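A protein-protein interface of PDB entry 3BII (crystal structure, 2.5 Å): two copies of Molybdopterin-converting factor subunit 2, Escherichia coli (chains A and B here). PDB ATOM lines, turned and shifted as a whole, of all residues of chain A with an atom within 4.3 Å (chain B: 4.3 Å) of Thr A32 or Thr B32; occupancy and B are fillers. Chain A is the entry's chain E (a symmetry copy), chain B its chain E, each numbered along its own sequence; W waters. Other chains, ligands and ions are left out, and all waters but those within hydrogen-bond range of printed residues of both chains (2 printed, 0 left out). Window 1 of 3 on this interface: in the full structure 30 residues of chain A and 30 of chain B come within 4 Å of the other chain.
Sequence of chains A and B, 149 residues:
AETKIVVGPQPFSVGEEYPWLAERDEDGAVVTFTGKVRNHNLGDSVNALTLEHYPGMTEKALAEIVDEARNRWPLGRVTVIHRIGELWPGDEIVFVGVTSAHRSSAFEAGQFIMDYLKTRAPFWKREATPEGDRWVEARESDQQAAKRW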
ATOM      1  N   TYR A  18     -17.064   0.618 -11.931  1.00  0.00           N
ATOM      2  CA  TYR A  18     -18.075  -0.302 -12.376  1.00  0.00           C
ATOM      3  C   TYR A  18     -18.163  -1.709 -11.707  1.00  0.00           C
ATOM      4  O   TYR A  18     -19.271  -2.128 -11.340  1.00  0.00           O
ATOM      5  CB  TYR A  18     -18.021  -0.412 -13.887  1.00  0.00           C
ATOM      6  CG  TYR A  18     -19.103  -1.294 -14.357  1.00  0.00           C
ATOM      7  CD1 TYR A  18     -20.384  -0.799 -14.597  1.00  0.00           C
ATOM      8  CD2 TYR A  18     -18.866  -2.648 -14.510  1.00  0.00           C
ATOM      9  CE1 TYR A  18     -21.394  -1.646 -15.019  1.00  0.00           C
ATOM     10  CE2 TYR A  18     -19.854  -3.494 -14.905  1.00  0.00           C
ATOM     11  CZ  TYR A  18     -21.111  -3.002 -15.163  1.00  0.00           C
ATOM     12  OH  TYR A  18     -22.062  -3.916 -15.544  1.00  0.00           O
ATOM     13  N   LEU A  21     -19.760  -1.647  -8.435  1.00  0.00           N
ATOM     14  CA  LEU A  21     -21.186  -1.383  -8.582  1.00  0.00           C
ATOM     15  C   LEU A  21     -21.967  -2.649  -8.950  1.00  0.00           C
ATOM     16  O   LEU A  21     -23.031  -2.899  -8.391  1.00  0.00           O
ATOM     17  CB  LEU A  21     -21.432  -0.257  -9.598  1.00  0.00           C
ATOM     18  CG  LEU A  21     -22.864   0.269  -9.813  1.00  0.00           C
ATOM     19  CD1 LEU A  21     -23.399   1.064  -8.597  1.00  0.00           C
ATOM     20  CD2 LEU A  21     -22.940   1.107 -11.112  1.00  0.00           C
ATOM     21  N   VAL A  30     -27.930  -3.083 -13.859  1.00  0.00           N
ATOM     22  CA  VAL A  30     -27.006  -1.983 -13.564  1.00  0.00           C
ATOM     23  C   VAL A  30     -27.110  -0.831 -14.572  1.00  0.00           C
ATOM     24  O   VAL A  30     -26.754  -0.997 -15.728  1.00  0.00           O
ATOM     25  CB  VAL A  30     -25.530  -2.491 -13.522  1.00  0.00           C
ATOM     26  CG1 VAL A  30     -24.572  -1.335 -13.323  1.00  0.00           C
ATOM     27  CG2 VAL A  30     -25.333  -3.537 -12.426  1.00  0.00           C
ATOM     28  N   VAL A  31     -27.590   0.326 -14.121  1.00  0.00           N
ATOM     29  CA  VAL A  31     -27.614   1.565 -14.920  1.00  0.00           C
ATOM     30  C   VAL A  31     -26.493   2.509 -14.498  1.00  0.00           C
ATOM     31  O   VAL A  31     -26.395   2.780 -13.318  1.00  0.00           O
ATOM     32  CB  VAL A  31     -28.965   2.277 -14.728  1.00  0.00           C
ATOM     33  CG1 VAL A  31     -28.977   3.670 -15.327  1.00  0.00           C
ATOM     34  CG2 VAL A  31     -30.067   1.435 -15.368  1.00  0.00           C
ATOM     35  N   THR A  32     -25.623   2.976 -15.415  1.00  0.00           N
ATOM     36  CA  THR A  32     -24.767   4.135 -15.100  1.00  0.00           C
ATOM     37  C   THR A  32     -25.130   5.379 -15.899  1.00  0.00           C
ATOM     38  O   THR A  32     -25.675   5.280 -17.011  1.00  0.00           O
ATOM     39  CB  THR A  32     -23.230   3.897 -15.237  1.00  0.00           C
ATOM     40  OG1 THR A  32     -22.825   3.973 -16.601  1.00  0.00           O
ATOM     41  CG2 THR A  32     -22.815   2.568 -14.652  1.00  0.00           C
ATOM     42  N   PHE A  33     -24.860   6.549 -15.318  1.00  0.00           N
ATOM     43  CA  PHE A  33     -24.893   7.797 -16.063  1.00  0.00           C
ATOM     44  C   PHE A  33     -23.574   8.554 -15.869  1.00  0.00           C
ATOM     45  O   PHE A  33     -23.052   8.624 -14.768  1.00  0.00           O
ATOM     46  CB  PHE A  33     -26.084   8.691 -15.665  1.00  0.00           C
ATOM     47  CG  PHE A  33     -26.055  10.071 -16.316  1.00  0.00           C
ATOM     48  CD1 PHE A  33     -26.676  10.284 -17.552  1.00  0.00           C
ATOM     49  CD2 PHE A  33     -25.374  11.141 -15.705  1.00  0.00           C
ATOM     50  CE1 PHE A  33     -26.644  11.537 -18.180  1.00  0.00           C
ATOM     51  CE2 PHE A  33     -25.340  12.424 -16.330  1.00  0.00           C
ATOM     52  CZ  PHE A  33     -25.985  12.615 -17.580  1.00  0.00           C
ATOM     53  N   PHE A  95     -20.478  11.041 -12.048  1.00  0.00           N
ATOM     54  CA  PHE A  95     -20.829   9.661 -12.256  1.00  0.00           C
ATOM     55  C   PHE A  95     -21.958   9.259 -11.321  1.00  0.00           C
ATOM     56  O   PHE A  95     -21.910   9.549 -10.116  1.00  0.00           O
ATOM     57  CB  PHE A  95     -19.632   8.753 -12.020  1.00  0.00           C
ATOM     58  CG  PHE A  95     -19.935   7.297 -12.259  1.00  0.00           C
ATOM     59  CD1 PHE A  95     -20.125   6.814 -13.559  1.00  0.00           C
ATOM     60  CD2 PHE A  95     -20.038   6.415 -11.194  1.00  0.00           C
ATOM     61  CE1 PHE A  95     -20.383   5.505 -13.789  1.00  0.00           C
ATOM     62  CE2 PHE A  95     -20.326   5.070 -11.422  1.00  0.00           C
ATOM     63  CZ  PHE A  95     -20.502   4.615 -12.719  1.00  0.00           C
ATOM     64  N   VAL A  96     -22.959   8.596 -11.879  1.00  0.00           N
ATOM     65  CA  VAL A  96     -24.060   8.032 -11.092  1.00  0.00           C
ATOM     66  C   VAL A  96     -24.210   6.558 -11.491  1.00  0.00           C
ATOM     67  O   VAL A  96     -24.281   6.239 -12.692  1.00  0.00           O
ATOM     68  CB  VAL A  96     -25.412   8.819 -11.294  1.00  0.00           C
ATOM     69  CG1 VAL A  96     -26.578   8.030 -10.741  1.00  0.00           C
ATOM     70  CG2 VAL A  96     -25.352  10.194 -10.658  1.00  0.00           C
ATOM     71  N   TYR B  18     -16.646   1.022 -22.563  1.00  0.00           N
ATOM     72  CA  TYR B  18     -16.990   2.357 -22.155  1.00  0.00           C
ATOM     73  C   TYR B  18     -16.241   3.562 -22.806  1.00  0.00           C
ATOM     74  O   TYR B  18     -16.905   4.523 -23.221  1.00  0.00           O
ATOM     75  CB  TYR B  18     -16.960   2.441 -20.642  1.00  0.00           C
ATOM     76  CG  TYR B  18     -17.385   3.785 -20.213  1.00  0.00           C
ATOM     77  CD1 TYR B  18     -18.734   4.096 -20.046  1.00  0.00           C
ATOM     78  CD2 TYR B  18     -16.438   4.777 -20.028  1.00  0.00           C
ATOM     79  CE1 TYR B  18     -19.115   5.370 -19.662  1.00  0.00           C
ATOM     80  CE2 TYR B  18     -16.801   6.037 -19.670  1.00  0.00           C
ATOM     81  CZ  TYR B  18     -18.129   6.337 -19.483  1.00  0.00           C
ATOM     82  OH  TYR B  18     -18.423   7.632 -19.136  1.00  0.00           O
ATOM     83  N   LEU B  21     -17.432   4.355 -26.155  1.00  0.00           N
ATOM     84  CA  LEU B  21     -18.767   4.936 -26.083  1.00  0.00           C
ATOM     85  C   LEU B  21     -18.722   6.428 -25.736  1.00  0.00           C
ATOM     86  O   LEU B  21     -19.434   7.223 -26.344  1.00  0.00           O
ATOM     87  CB  LEU B  21     -19.652   4.157 -25.099  1.00  0.00           C
ATOM     88  CG  LEU B  21     -21.141   4.527 -24.965  1.00  0.00           C
ATOM     89  CD1 LEU B  21     -21.968   4.149 -26.218  1.00  0.00           C
ATOM     90  CD2 LEU B  21     -21.739   3.895 -23.684  1.00  0.00           C
ATOM     91  N   VAL B  30     -23.657  10.202 -21.128  1.00  0.00           N
ATOM     92  CA  VAL B  30     -23.494   8.770 -21.393  1.00  0.00           C
ATOM     93  C   VAL B  30     -24.276   7.889 -20.409  1.00  0.00           C
ATOM     94  O   VAL B  30     -23.947   7.845 -19.234  1.00  0.00           O
ATOM     95  CB  VAL B  30     -21.987   8.364 -21.352  1.00  0.00           C
ATOM     96  CG1 VAL B  30     -21.832   6.867 -21.521  1.00  0.00           C
ATOM     97  CG2 VAL B  30     -21.184   9.102 -22.421  1.00  0.00           C
ATOM     98  N   VAL B  31     -25.298   7.193 -20.901  1.00  0.00           N
ATOM     99  CA  VAL B  31     -26.052   6.192 -20.123  1.00  0.00           C
ATOM    100  C   VAL B  31     -25.633   4.776 -20.503  1.00  0.00           C
ATOM    101  O   VAL B  31     -25.644   4.479 -21.681  1.00  0.00           O
ATOM    102  CB  VAL B  31     -27.559   6.356 -20.394  1.00  0.00           C
ATOM    103  CG1 VAL B  31     -28.379   5.218 -19.819  1.00  0.00           C
ATOM    104  CG2 VAL B  31     -28.030   7.680 -19.798  1.00  0.00           C
ATOM    105  N   THR B  32     -25.220   3.916 -19.551  1.00  0.00           N
ATOM    106  CA  THR B  32     -25.147   2.472 -19.840  1.00  0.00           C
ATOM    107  C   THR B  32     -26.183   1.657 -19.080  1.00  0.00           C
ATOM    108  O   THR B  32     -26.634   2.061 -17.995  1.00  0.00           O
ATOM    109  CB  THR B  32     -23.749   1.810 -19.623  1.00  0.00           C
ATOM    110  OG1 THR B  32     -23.526   1.541 -18.241  1.00  0.00           O
ATOM    111  CG2 THR B  32     -22.632   2.669 -20.165  1.00  0.00           C
ATOM    112  N   PHE B  33     -26.587   0.527 -19.664  1.00  0.00           N
ATOM    113  CA  PHE B  33     -27.350  -0.477 -18.942  1.00  0.00           C
ATOM    114  C   PHE B  33     -26.673  -1.845 -19.080  1.00  0.00           C
ATOM    115  O   PHE B  33     -26.225  -2.212 -20.155  1.00  0.00           O
ATOM    116  CB  PHE B  33     -28.815  -0.556 -19.413  1.00  0.00           C
ATOM    117  CG  PHE B  33     -29.597  -1.705 -18.783  1.00  0.00           C
ATOM    118  CD1 PHE B  33     -30.292  -1.515 -17.583  1.00  0.00           C
ATOM    119  CD2 PHE B  33     -29.602  -2.983 -19.375  1.00  0.00           C
ATOM    120  CE1 PHE B  33     -30.998  -2.561 -16.973  1.00  0.00           C
ATOM    121  CE2 PHE B  33     -30.324  -4.054 -18.769  1.00  0.00           C
ATOM    122  CZ  PHE B  33     -31.028  -3.832 -17.556  1.00  0.00           C
ATOM    123  N   PHE B  95     -25.313  -5.698 -22.778  1.00  0.00           N
ATOM    124  CA  PHE B  95     -24.841  -4.355 -22.567  1.00  0.00           C
ATOM    125  C   PHE B  95     -25.502  -3.404 -23.552  1.00  0.00           C
ATOM    126  O   PHE B  95     -25.565  -3.690 -24.757  1.00  0.00           O
ATOM    127  CB  PHE B  95     -23.331  -4.277 -22.729  1.00  0.00           C
ATOM    128  CG  PHE B  95     -22.778  -2.897 -22.483  1.00  0.00           C
ATOM    129  CD1 PHE B  95     -22.730  -2.371 -21.187  1.00  0.00           C
ATOM    130  CD2 PHE B  95     -22.316  -2.125 -23.538  1.00  0.00           C
ATOM    131  CE1 PHE B  95     -22.222  -1.138 -20.950  1.00  0.00           C
ATOM    132  CE2 PHE B  95     -21.812  -0.847 -23.304  1.00  0.00           C
ATOM    133  CZ  PHE B  95     -21.768  -0.351 -22.011  1.00  0.00           C
ATOM    134  N   VAL B  96     -25.987  -2.285 -23.035  1.00  0.00           N
ATOM    135  CA  VAL B  96     -26.542  -1.214 -23.867  1.00  0.00           C
ATOM    136  C   VAL B  96     -25.861   0.097 -23.454  1.00  0.00           C
ATOM    137  O   VAL B  96     -25.801   0.420 -22.253  1.00  0.00           O
ATOM    138  CB  VAL B  96     -28.111  -1.105 -23.745  1.00  0.00           C
ATOM    139  CG1 VAL B  96     -28.606   0.192 -24.345  1.00  0.00           C
ATOM    140  CG2 VAL B  96     -28.800  -2.288 -24.399  1.00  0.00           C
HETATM  141  O   HOH W   1     -24.330  -0.403 -16.768  1.00  0.00           O
HETATM  142  O   HOH W   2     -22.327   6.012 -18.083  1.00  0.00           O
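The backbone NH of Thr A32 is in hydrogen-bond range of the backbone carbonyl oxygen of Thr B32, at 2.9 Å.
The backbone carbonyl oxygen of Val B96 sits at hydrogen-bond distance from the backbone NH of Phe B33 (2.7 Å).
The backbone NH (N) of Phe A33 is in hydrogen-bond range of the backbone carbonyl oxygen (O) of Val A96, at 2.7 Å.
Thr B32 touches Val A30 (O to O, 3.8 Å).
Val A30 touches Phe B33 (O to CA, 3.3 Å).
CA of Val A31 touches O of Thr B32, 3.3 Å away.
CD1 of Phe B33 touches CG2 of Val A31, 3.7 Å away.
Thr A32 touches Val B30.
Thr A32 touches Val B31.
Val B30 touches Phe A33 (O to CA, 3.3 Å).
Phe A33 touches Val B31.
Of the printed residues of chain B, Val A31 touches Thr B32 and Phe B33.
Thr A32 touches just these residues of chain B: Val B30 (3.8 Å), Val B31 (3.3 Å) and Thr B32 (2.9 Å).
Of the printed residues of chain B, Phe A33 touches Val B30 (3.3 Å) and Val B31 (3.7 Å).
Of the printed residues of chain A, Val B30 touches Thr A32 (3.8 Å) and Phe A33 (3.3 Å).
Of the printed residues of chain A, Val B31 touches Thr A32 (3.3 Å) and Phe A33 (3.7 Å).
Of chain A, only Val A30, Val A31 and Thr A32 come within 4 Å of Thr B32.
Phe B95 touches none of the printed residues of chain A.
The nearest printed residue of chain B that does not touch Thr A32 is Phe B33 (5.0 Å).
The nearest printed residue of chain B that does not touch Val A31 is Val B31 (4.8 Å).
Of the 8 printed residues of chain A, 4 touch a printed residue of chain B.
Printed residues of chain A that touch a printed residue of chain B: Val A30, Val A31, Thr A32 and Phe A33.
Along chain A the printed residues that touch a printed residue of chain B span positions 30 to 33.
Of the 8 printed residues of chain B, 4 touch a printed residue of chain A.
Hydrophobic or aromatic side chains of chain B within 4 Å of the printed part of chain A: Val B31 and Phe B33.
Among the printed residues, 9 pairs touch across the chains.
Among the printed residues, no Asp or Glu carboxylate lies within 4 Å of a Lys or Arg side-chain nitrogen of the other chain.
Val A30 touches Thr B32, and with the chains exchanged Thr A32 touches Val B30.
Val A30 touches Phe B33, and with the chains exchanged Phe A33 touches Val B30.
Val A31 touches Phe B33, and with the chains exchanged Phe A33 touches Val B31.
Thr A32 touches its own counterpart, Thr B32.
8 positions are printed for both chains.
Water W2 bridges the side-chain hydroxyl of Thr A32 (2.6 Å) and the backbone carbonyl oxygen of Val B30 (2.7 Å).
Water W1 bridges the side-chain hydroxyl of Thr B32 (2.6 Å) and the backbone carbonyl oxygen of Val A30 (2.7 Å).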
